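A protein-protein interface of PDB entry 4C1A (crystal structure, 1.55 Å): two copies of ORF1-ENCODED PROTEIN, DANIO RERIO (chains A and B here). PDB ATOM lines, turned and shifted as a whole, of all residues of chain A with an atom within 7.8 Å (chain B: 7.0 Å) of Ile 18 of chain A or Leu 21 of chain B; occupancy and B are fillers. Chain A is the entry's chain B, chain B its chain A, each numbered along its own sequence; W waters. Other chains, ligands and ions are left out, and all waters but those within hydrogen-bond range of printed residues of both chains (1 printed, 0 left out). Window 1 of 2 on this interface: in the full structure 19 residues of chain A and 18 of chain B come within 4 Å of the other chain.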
ATOM      1  N   LEU A  11      11.265  13.860 -30.150  1.00  0.00           N
ATOM      2  CA  LEU A  11      11.567  12.774 -29.199  1.00  0.00           C
ATOM      3  C   LEU A  11      11.158  11.392 -29.744  1.00  0.00           C
ATOM      4  O   LEU A  11      11.884  10.408 -29.582  1.00  0.00           O
ATOM      5  CB  LEU A  11      10.897  13.051 -27.857  1.00  0.00           C
ATOM      6  CG  LEU A  11      11.715  13.963 -26.959  1.00  0.00           C
ATOM      7  CD1 LEU A  11      10.844  14.494 -25.873  1.00  0.00           C
ATOM      8  CD2 LEU A  11      12.858  13.190 -26.377  1.00  0.00           C
ATOM      9  N   GLU A  12      10.018  11.313 -30.429  1.00  0.00           N
ATOM     10  CA  GLU A  12       9.637  10.056 -31.071  1.00  0.00           C
ATOM     11  C   GLU A  12      10.639   9.612 -32.144  1.00  0.00           C
ATOM     12  O   GLU A  12      10.960   8.430 -32.256  1.00  0.00           O
ATOM     13  CB  GLU A  12       8.277  10.177 -31.754  1.00  0.00           C
ATOM     14  CG  GLU A  12       7.107  10.102 -30.858  1.00  0.00           C
ATOM     15  CD  GLU A  12       5.863   9.781 -31.667  1.00  0.00           C
ATOM     16  OE1 GLU A  12       5.367  10.674 -32.384  1.00  0.00           O
ATOM     17  OE2 GLU A  12       5.427   8.617 -31.633  1.00  0.00           O
ATOM     18  N   GLU A  13      11.085  10.562 -32.959  1.00  0.00           N
ATOM     19  CA  GLU A  13      12.078  10.311 -33.988  1.00  0.00           C
ATOM     20  C   GLU A  13      13.372   9.784 -33.381  1.00  0.00           C
ATOM     21  O   GLU A  13      13.885   8.743 -33.826  1.00  0.00           O
ATOM     22  CB  GLU A  13      12.343  11.587 -34.775  1.00  0.00           C
ATOM     23  CG  GLU A  13      11.191  12.022 -35.646  1.00  0.00           C
ATOM     24  CD  GLU A  13      11.426  13.375 -36.271  1.00  0.00           C
ATOM     25  OE1 GLU A  13      12.434  14.034 -35.947  1.00  0.00           O
ATOM     26  OE2 GLU A  13      10.610  13.776 -37.107  1.00  0.00           O
ATOM     27  N   VAL A  14      13.891  10.465 -32.370  1.00  0.00           N
ATOM     28  CA  VAL A  14      15.134  10.060 -31.742  1.00  0.00           C
ATOM     29  C   VAL A  14      14.997   8.706 -31.113  1.00  0.00           C
ATOM     30  O   VAL A  14      15.899   7.868 -31.224  1.00  0.00           O
ATOM     31  CB  VAL A  14      15.660  11.111 -30.699  1.00  0.00           C
ATOM     32  CG1 VAL A  14      14.707  11.323 -29.591  1.00  0.00           C
ATOM     33  CG2 VAL A  14      16.974  10.685 -30.095  1.00  0.00           C
ATOM     34  N   GLU A  15      13.871   8.457 -30.446  1.00  0.00           N
ATOM     35  CA  GLU A  15      13.682   7.134 -29.855  1.00  0.00           C
ATOM     36  C   GLU A  15      13.655   6.015 -30.879  1.00  0.00           C
ATOM     37  O   GLU A  15      14.234   4.962 -30.634  1.00  0.00           O
ATOM     38  CB  GLU A  15      12.401   7.115 -29.022  1.00  0.00           C
ATOM     39  CG  GLU A  15      12.342   5.956 -28.049  1.00  0.00           C
ATOM     40  CD  GLU A  15      13.424   6.013 -26.978  1.00  0.00           C
ATOM     41  OE1 GLU A  15      13.925   7.113 -26.692  1.00  0.00           O
ATOM     42  OE2 GLU A  15      13.774   4.943 -26.437  1.00  0.00           O
ATOM     43  N   SER A  16      13.006   6.228 -32.022  1.00  0.00           N
ATOM     44  CA  SER A  16      12.944   5.198 -33.056  1.00  0.00           C
ATOM     45  C   SER A  16      14.356   4.899 -33.544  1.00  0.00           C
ATOM     46  O   SER A  16      14.725   3.721 -33.732  1.00  0.00           O
ATOM     47  CB  SER A  16      12.076   5.610 -34.237  1.00  0.00           C
ATOM     48  OG  SER A  16      10.722   5.457 -33.905  1.00  0.00           O
ATOM     49  N   GLN A  17      15.141   5.961 -33.745  1.00  0.00           N
ATOM     50  CA  GLN A  17      16.526   5.831 -34.207  1.00  0.00           C
ATOM     51  C   GLN A  17      17.374   5.078 -33.179  1.00  0.00           C
ATOM     52  O   GLN A  17      18.189   4.209 -33.528  1.00  0.00           O
ATOM     53  CB  GLN A  17      17.137   7.201 -34.463  1.00  0.00           C
ATOM     54  CG  GLN A  17      16.667   7.929 -35.703  1.00  0.00           C
ATOM     55  CD  GLN A  17      17.429   9.231 -35.863  1.00  0.00           C
ATOM     56  OE1 GLN A  17      18.567   9.245 -36.341  1.00  0.00           O
ATOM     57  NE2 GLN A  17      16.832  10.319 -35.410  1.00  0.00           N
ATOM     58  N   ILE A  18      17.203   5.416 -31.900  1.00  0.00           N
ATOM     59  CA  ILE A  18      17.940   4.721 -30.843  1.00  0.00           C
ATOM     60  C   ILE A  18      17.565   3.256 -30.820  1.00  0.00           C
ATOM     61  O   ILE A  18      18.425   2.379 -30.715  1.00  0.00           O
ATOM     62  CB  ILE A  18      17.733   5.365 -29.480  1.00  0.00           C
ATOM     63  CG1 ILE A  18      18.429   6.720 -29.398  1.00  0.00           C
ATOM     64  CG2 ILE A  18      18.263   4.472 -28.345  1.00  0.00           C
ATOM     65  CD1 ILE A  18      17.946   7.566 -28.208  1.00  0.00           C
ATOM     66  N   ARG A  19      16.274   2.971 -30.906  1.00  0.00           N
ATOM     67  CA  ARG A  19      15.852   1.592 -30.817  1.00  0.00           C
ATOM     68  C   ARG A  19      16.491   0.760 -31.942  1.00  0.00           C
ATOM     69  O   ARG A  19      16.891  -0.367 -31.701  1.00  0.00           O
ATOM     70  CB  ARG A  19      14.349   1.480 -30.837  1.00  0.00           C
ATOM     71  CG  ARG A  19      13.735   1.961 -29.535  1.00  0.00           C
ATOM     72  CD  ARG A  19      12.312   1.481 -29.406  1.00  0.00           C
ATOM     73  NE  ARG A  19      11.466   2.203 -30.337  1.00  0.00           N
ATOM     74  CZ  ARG A  19      10.586   3.138 -29.993  1.00  0.00           C
ATOM     75  NH1 ARG A  19      10.391   3.458 -28.716  1.00  0.00           N
ATOM     76  NH2 ARG A  19       9.880   3.742 -30.940  1.00  0.00           N
ATOM     77  N   ALA A  20      16.576   1.322 -33.144  1.00  0.00           N
ATOM     78  CA  ALA A  20      17.135   0.593 -34.287  1.00  0.00           C
ATOM     79  C   ALA A  20      18.630   0.366 -34.108  1.00  0.00           C
ATOM     80  O   ALA A  20      19.160  -0.734 -34.386  1.00  0.00           O
ATOM     81  CB  ALA A  20      16.865   1.345 -35.585  1.00  0.00           C
ATOM     82  N   LEU A  21      19.312   1.383 -33.610  1.00  0.00           N
ATOM     83  CA  LEU A  21      20.734   1.268 -33.361  1.00  0.00           C
ATOM     84  C   LEU A  21      21.051   0.300 -32.252  1.00  0.00           C
ATOM     85  O   LEU A  21      22.036  -0.470 -32.334  1.00  0.00           O
ATOM     86  CB  LEU A  21      21.374   2.620 -33.076  1.00  0.00           C
ATOM     87  CG  LEU A  21      21.433   3.546 -34.286  1.00  0.00           C
ATOM     88  CD1 LEU A  21      21.874   4.889 -33.811  1.00  0.00           C
ATOM     89  CD2 LEU A  21      22.378   2.999 -35.343  1.00  0.00           C
ATOM     90  N   VAL A  22      20.196   0.246 -31.224  1.00  0.00           N
ATOM     91  CA  VAL A  22      20.360  -0.730 -30.140  1.00  0.00           C
ATOM     92  C   VAL A  22      20.218  -2.171 -30.663  1.00  0.00           C
ATOM     93  O   VAL A  22      20.945  -3.056 -30.245  1.00  0.00           O
ATOM     94  CB  VAL A  22      19.322  -0.450 -29.032  1.00  0.00           C
ATOM     95  CG1 VAL A  22      19.171  -1.604 -28.111  1.00  0.00           C
ATOM     96  CG2 VAL A  22      19.747   0.742 -28.228  1.00  0.00           C
ATOM     97  N   VAL A  23      19.264  -2.418 -31.570  1.00  0.00           N
ATOM     98  CA  VAL A  23      19.147  -3.737 -32.183  1.00  0.00           C
ATOM     99  C   VAL A  23      20.411  -4.125 -32.965  1.00  0.00           C
ATOM    100  O   VAL A  23      20.921  -5.280 -32.866  1.00  0.00           O
ATOM    101  CB  VAL A  23      17.914  -3.783 -33.091  1.00  0.00           C
ATOM    102  CG1 VAL A  23      17.846  -5.057 -33.862  1.00  0.00           C
ATOM    103  CG2 VAL A  23      16.692  -3.629 -32.237  1.00  0.00           C
ATOM    104  N   ARG A  24      20.974  -3.160 -33.674  1.00  0.00           N
ATOM    105  CA  ARG A  24      22.185  -3.416 -34.435  1.00  0.00           C
ATOM    106  C   ARG A  24      23.349  -3.717 -33.496  1.00  0.00           C
ATOM    107  O   ARG A  24      24.129  -4.656 -33.713  1.00  0.00           O
ATOM    108  CB  ARG A  24      22.509  -2.216 -35.332  1.00  0.00           C
ATOM    109  CG  ARG A  24      23.798  -2.378 -36.093  1.00  0.00           C
ATOM    110  CD  ARG A  24      23.808  -1.479 -37.323  1.00  0.00           C
ATOM    111  NE  ARG A  24      25.116  -1.408 -37.968  1.00  0.00           N
ATOM    112  CZ  ARG A  24      25.643  -2.360 -38.722  1.00  0.00           C
ATOM    113  NH1 ARG A  24      24.990  -3.496 -38.921  1.00  0.00           N
ATOM    114  NH2 ARG A  24      26.843  -2.170 -39.276  1.00  0.00           N
ATOM    115  N   ARG A  25      23.465  -2.917 -32.446  1.00  0.00           N
ATOM    116  CA  ARG A  25      24.487  -3.121 -31.431  1.00  0.00           C
ATOM    117  C   ARG A  25      24.435  -4.540 -30.886  1.00  0.00           C
ATOM    118  O   ARG A  25      25.456  -5.193 -30.754  1.00  0.00           O
ATOM    119  CB  ARG A  25      24.330  -2.088 -30.318  1.00  0.00           C
ATOM    120  CG  ARG A  25      25.435  -2.002 -29.329  1.00  0.00           C
ATOM    121  CD  ARG A  25      25.164  -0.852 -28.378  1.00  0.00           C
ATOM    122  NE  ARG A  25      24.008  -1.152 -27.547  1.00  0.00           N
ATOM    123  CZ  ARG A  25      23.445  -0.307 -26.686  1.00  0.00           C
ATOM    124  NH1 ARG A  25      23.916   0.927 -26.520  1.00  0.00           N
ATOM    125  NH2 ARG A  25      22.396  -0.691 -25.990  1.00  0.00           N
ATOM    126  N   SER B  16      29.017   4.974 -30.437  1.00  0.00           N
ATOM    127  CA  SER B  16      29.155   6.422 -30.496  1.00  0.00           C
ATOM    128  C   SER B  16      27.894   7.133 -30.998  1.00  0.00           C
ATOM    129  O   SER B  16      27.524   8.188 -30.458  1.00  0.00           O
ATOM    130  CB  SER B  16      30.335   6.799 -31.376  1.00  0.00           C
ATOM    131  OG  SER B  16      31.518   6.303 -30.795  1.00  0.00           O
ATOM    132  N   GLN B  17      27.230   6.574 -32.012  1.00  0.00           N
ATOM    133  CA  GLN B  17      26.005   7.158 -32.558  1.00  0.00           C
ATOM    134  C   GLN B  17      24.892   7.096 -31.514  1.00  0.00           C
ATOM    135  O   GLN B  17      24.090   8.028 -31.394  1.00  0.00           O
ATOM    136  CB  GLN B  17      25.539   6.428 -33.821  1.00  0.00           C
ATOM    137  CG  GLN B  17      26.419   6.559 -35.096  1.00  0.00           C
ATOM    138  CD  GLN B  17      25.874   5.675 -36.209  1.00  0.00           C
ATOM    139  OE1 GLN B  17      26.267   4.520 -36.349  1.00  0.00           O
ATOM    140  NE2 GLN B  17      24.918   6.200 -36.967  1.00  0.00           N
ATOM    141  N   ILE B  18      24.815   5.992 -30.792  1.00  0.00           N
ATOM    142  CA  ILE B  18      23.805   5.878 -29.729  1.00  0.00           C
ATOM    143  C   ILE B  18      24.085   6.915 -28.672  1.00  0.00           C
ATOM    144  O   ILE B  18      23.153   7.565 -28.193  1.00  0.00           O
ATOM    145  CB  ILE B  18      23.736   4.456 -29.130  1.00  0.00           C
ATOM    146  CG1 ILE B  18      23.163   3.493 -30.167  1.00  0.00           C
ATOM    147  CG2 ILE B  18      22.879   4.430 -27.849  1.00  0.00           C
ATOM    148  CD1 ILE B  18      23.399   2.029 -29.868  1.00  0.00           C
ATOM    149  N   ARG B  19      25.346   7.105 -28.297  1.00  0.00           N
ATOM    150  CA  ARG B  19      25.636   8.037 -27.196  1.00  0.00           C
ATOM    151  C   ARG B  19      25.204   9.426 -27.578  1.00  0.00           C
ATOM    152  O   ARG B  19      24.658  10.147 -26.769  1.00  0.00           O
ATOM    153  CB  ARG B  19      27.125   8.059 -26.823  1.00  0.00           C
ATOM    154  CG  ARG B  19      27.575   6.870 -25.998  1.00  0.00           C
ATOM    155  CD  ARG B  19      28.964   7.095 -25.408  1.00  0.00           C
ATOM    156  NE  ARG B  19      30.022   7.008 -26.416  1.00  0.00           N
ATOM    157  CZ  ARG B  19      30.756   5.922 -26.655  1.00  0.00           C
ATOM    158  NH1 ARG B  19      30.572   4.805 -25.957  1.00  0.00           N
ATOM    159  NH2 ARG B  19      31.691   5.959 -27.600  1.00  0.00           N
ATOM    160  N   ALA B  20      25.440   9.787 -28.832  1.00  0.00           N
ATOM    161  CA  ALA B  20      25.050  11.100 -29.356  1.00  0.00           C
ATOM    162  C   ALA B  20      23.534  11.310 -29.364  1.00  0.00           C
ATOM    163  O   ALA B  20      23.059  12.402 -28.992  1.00  0.00           O
ATOM    164  CB  ALA B  20      25.646  11.283 -30.757  1.00  0.00           C
ATOM    165  N   LEU B  21      22.781  10.271 -29.756  1.00  0.00           N
ATOM    166  CA  LEU B  21      21.341  10.328 -29.774  1.00  0.00           C
ATOM    167  C   LEU B  21      20.788  10.437 -28.378  1.00  0.00           C
ATOM    168  O   LEU B  21      19.826  11.164 -28.160  1.00  0.00           O
ATOM    169  CB  LEU B  21      20.737   9.139 -30.508  1.00  0.00           C
ATOM    170  CG  LEU B  21      20.926   9.226 -32.028  1.00  0.00           C
ATOM    171  CD1 LEU B  21      20.592   7.931 -32.666  1.00  0.00           C
ATOM    172  CD2 LEU B  21      20.029  10.304 -32.611  1.00  0.00           C
ATOM    173  N   VAL B  22      21.440   9.771 -27.429  1.00  0.00           N
ATOM    174  CA  VAL B  22      21.005   9.829 -26.044  1.00  0.00           C
ATOM    175  C   VAL B  22      21.220  11.215 -25.484  1.00  0.00           C
ATOM    176  O   VAL B  22      20.371  11.711 -24.743  1.00  0.00           O
ATOM    177  CB  VAL B  22      21.712   8.757 -25.174  1.00  0.00           C
ATOM    178  CG1 VAL B  22      21.459   9.021 -23.682  1.00  0.00           C
ATOM    179  CG2 VAL B  22      21.222   7.323 -25.559  1.00  0.00           C
ATOM    180  N   VAL B  23      22.332  11.875 -25.824  1.00  0.00           N
ATOM    181  CA  VAL B  23      22.523  13.274 -25.420  1.00  0.00           C
ATOM    182  C   VAL B  23      21.440  14.181 -25.994  1.00  0.00           C
ATOM    183  O   VAL B  23      20.929  15.031 -25.295  1.00  0.00           O
ATOM    184  CB  VAL B  23      23.898  13.775 -25.861  1.00  0.00           C
ATOM    185  CG1 VAL B  23      24.044  15.267 -25.709  1.00  0.00           C
ATOM    186  CG2 VAL B  23      24.929  13.079 -25.035  1.00  0.00           C
ATOM    187  N   ARG B  24      21.072  13.942 -27.254  1.00  0.00           N
ATOM    188  CA  ARG B  24      20.022  14.704 -27.904  1.00  0.00           C
ATOM    189  C   ARG B  24      18.673  14.471 -27.202  1.00  0.00           C
ATOM    190  O   ARG B  24      17.939  15.416 -26.914  1.00  0.00           O
ATOM    191  CB  ARG B  24      19.961  14.384 -29.390  1.00  0.00           C
ATOM    192  CG  ARG B  24      18.862  15.198 -30.073  1.00  0.00           C
ATOM    193  CD  ARG B  24      18.950  15.148 -31.591  1.00  0.00           C
ATOM    194  NE  ARG B  24      17.735  15.647 -32.243  1.00  0.00           N
ATOM    195  CZ  ARG B  24      17.301  16.904 -32.199  1.00  0.00           C
ATOM    196  NH1 ARG B  24      17.961  17.828 -31.521  1.00  0.00           N
ATOM    197  NH2 ARG B  24      16.182  17.236 -32.843  1.00  0.00           N
ATOM    198  N   ARG B  25      18.376  13.223 -26.888  1.00  0.00           N
ATOM    199  CA  ARG B  25      17.165  12.862 -26.201  1.00  0.00           C
ATOM    200  C   ARG B  25      17.123  13.577 -24.864  1.00  0.00           C
ATOM    201  O   ARG B  25      16.096  14.087 -24.491  1.00  0.00           O
ATOM    202  CB  ARG B  25      17.085  11.338 -26.020  1.00  0.00           C
ATOM    203  CG  ARG B  25      15.801  10.804 -25.474  1.00  0.00           C
ATOM    204  CD  ARG B  25      15.779   9.326 -25.427  1.00  0.00           C
ATOM    205  NE  ARG B  25      16.786   8.834 -24.500  1.00  0.00           N
ATOM    206  CZ  ARG B  25      17.120   7.570 -24.290  1.00  0.00           C
ATOM    207  NH1 ARG B  25      16.534   6.574 -24.941  1.00  0.00           N
ATOM    208  NH2 ARG B  25      18.051   7.316 -23.390  1.00  0.00           N
ATOM    209  N   SER B  26      18.238  13.609 -24.131  1.00  0.00           N
ATOM    210  CA  SER B  26      18.203  14.269 -22.832  1.00  0.00           C
ATOM    211  C   SER B  26      17.929  15.745 -22.997  1.00  0.00           C
ATOM    212  O   SER B  26      17.232  16.320 -22.187  1.00  0.00           O
ATOM    213  CB  SER B  26      19.536  14.127 -22.100  1.00  0.00           C
ATOM    214  OG  SER B  26      19.794  12.800 -21.711  1.00  0.00           O
ATOM    215  N   ARG B  27      18.506  16.358 -24.026  1.00  0.00           N
ATOM    216  CA  ARG B  27      18.344  17.779 -24.253  1.00  0.00           C
ATOM    217  C   ARG B  27      16.901  18.081 -24.637  1.00  0.00           C
ATOM    218  O   ARG B  27      16.297  19.040 -24.123  1.00  0.00           O
ATOM    219  CB  ARG B  27      19.282  18.244 -25.356  1.00  0.00           C
ATOM    220  CG  ARG B  27      20.713  18.506 -24.935  1.00  0.00           C
ATOM    221  CD  ARG B  27      21.577  18.824 -26.165  1.00  0.00           C
ATOM    222  NE  ARG B  27      23.006  18.835 -25.848  1.00  0.00           N
ATOM    223  CZ  ARG B  27      23.965  18.440 -26.685  1.00  0.00           C
ATOM    224  NH1 ARG B  27      23.664  17.994 -27.905  1.00  0.00           N
ATOM    225  NH2 ARG B  27      25.236  18.496 -26.298  1.00  0.00           N
ATOM    226  N   LEU B  28      16.311  17.245 -25.486  1.00  0.00           N
ATOM    227  CA  LEU B  28      14.938  17.464 -25.902  1.00  0.00           C
ATOM    228  C   LEU B  28      13.985  17.280 -24.722  1.00  0.00           C
ATOM    229  O   LEU B  28      13.039  18.063 -24.571  1.00  0.00           O
ATOM    230  CB  LEU B  28      14.526  16.508 -27.012  1.00  0.00           C
ATOM    231  CG  LEU B  28      15.126  16.777 -28.381  1.00  0.00           C
ATOM    232  CD1 LEU B  28      14.986  15.538 -29.210  1.00  0.00           C
ATOM    233  CD2 LEU B  28      14.448  17.933 -29.106  1.00  0.00           C
HETATM  234  O   HOH W   1      13.254   6.264 -23.810  1.00  0.00           O
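The guanidinium group (NH1) of Arg 25 of chain B is in salt-bridge range of the side-chain carboxylate (OE1) of Glu 15 of chain A, at 3.2 Å.
Gln 17 of chain A touches Leu 21 of chain B, and with the chains exchanged Leu 21 of chain A touches Gln 17 of chain B.
Ile 18 of chain A touches Leu 21 of chain B, and with the chains exchanged Leu 21 of chain A touches Ile 18 of chain B.
Ile 18 of chain A touches Arg 25 of chain B, and with the chains exchanged Arg 25 of chain A touches Ile 18 of chain B.
Val 22 of chain A touches Ile 18 of chain B, but with the chains exchanged Ile 18 of chain A does not touch Val 22 of chain B (4.2 Å).
10 positions are printed for both chains.
Among the printed residues, merely in contact across the chains: Val 14 of chain A with Leu 21 of chain B (3.5 Å), Leu 21 of chain A with Leu 21 of chain B (3.5 Å), Ile 18 of chain A with Leu 21 of chain B (3.5 Å), Leu 21 of chain A with Ile 18 of chain B (3.5 Å), Arg 25 of chain A with Ile 18 of chain B (3.6 Å), Ile 18 of chain A with Arg 25 of chain B (3.7 Å), Leu 11 of chain A with Leu 28 of chain B (3.8 Å), Leu 11 of chain A with Arg 25 of chain B (3.9 Å), Val 22 of chain A with Ile 18 of chain B (3.9 Å), Gln 17 of chain A with Leu 21 of chain B (3.96 Å) and Leu 21 of chain A with Gln 17 of chain B (3.98 Å).
Hydrophobic or aromatic side chains of chain B within 4 Å of the printed part of chain A: Ile 18, Leu 21 and Leu 28.
Along chain A the printed residues that touch a printed residue of chain B span positions 11 to 25.
Water W1 bridges OE2 of Glu 15 of chain A (3.0 Å) and NH1 of Arg 25 of chain B (3.5 Å).
Ile 18 of chain A touches two residues of chain B.
Of the printed residues of chain A, Leu 21 of chain B touches Val 14 (3.5 Å), Gln 17 (3.96 Å), Ile 18 (3.5 Å) and Leu 21 (3.5 Å).
No residue of chain A comes within 4 Å of Ala 20 of chain B.
Of the printed residues of chain B, Gln 17 of chain A touches Leu 21.
Of the printed residues of chain A, Ile 18 of chain B touches Leu 21 (3.5 Å), Val 22 (3.9 Å) and Arg 25 (3.6 Å).
Of the printed residues of chain B, Leu 11 of chain A touches Arg 25 and Leu 28.
Of the printed residues of chain B, Val 14 of chain A touches Leu 21 (3.5 Å).
Of the printed residues of chain B, Leu 21 of chain A touches Gln 17 (3.98 Å), Ile 18 (3.5 Å) and Leu 21 (3.5 Å).
Glu 12 of chain A touches none of the printed residues of chain B.
The nearest residue of chain B that does not touch Ile 18 of chain A is Val 22 of chain B (4.2 Å).
The nearest residue of chain A that does not touch Leu 21 of chain B is Glu 13 of chain A (6.5 Å).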
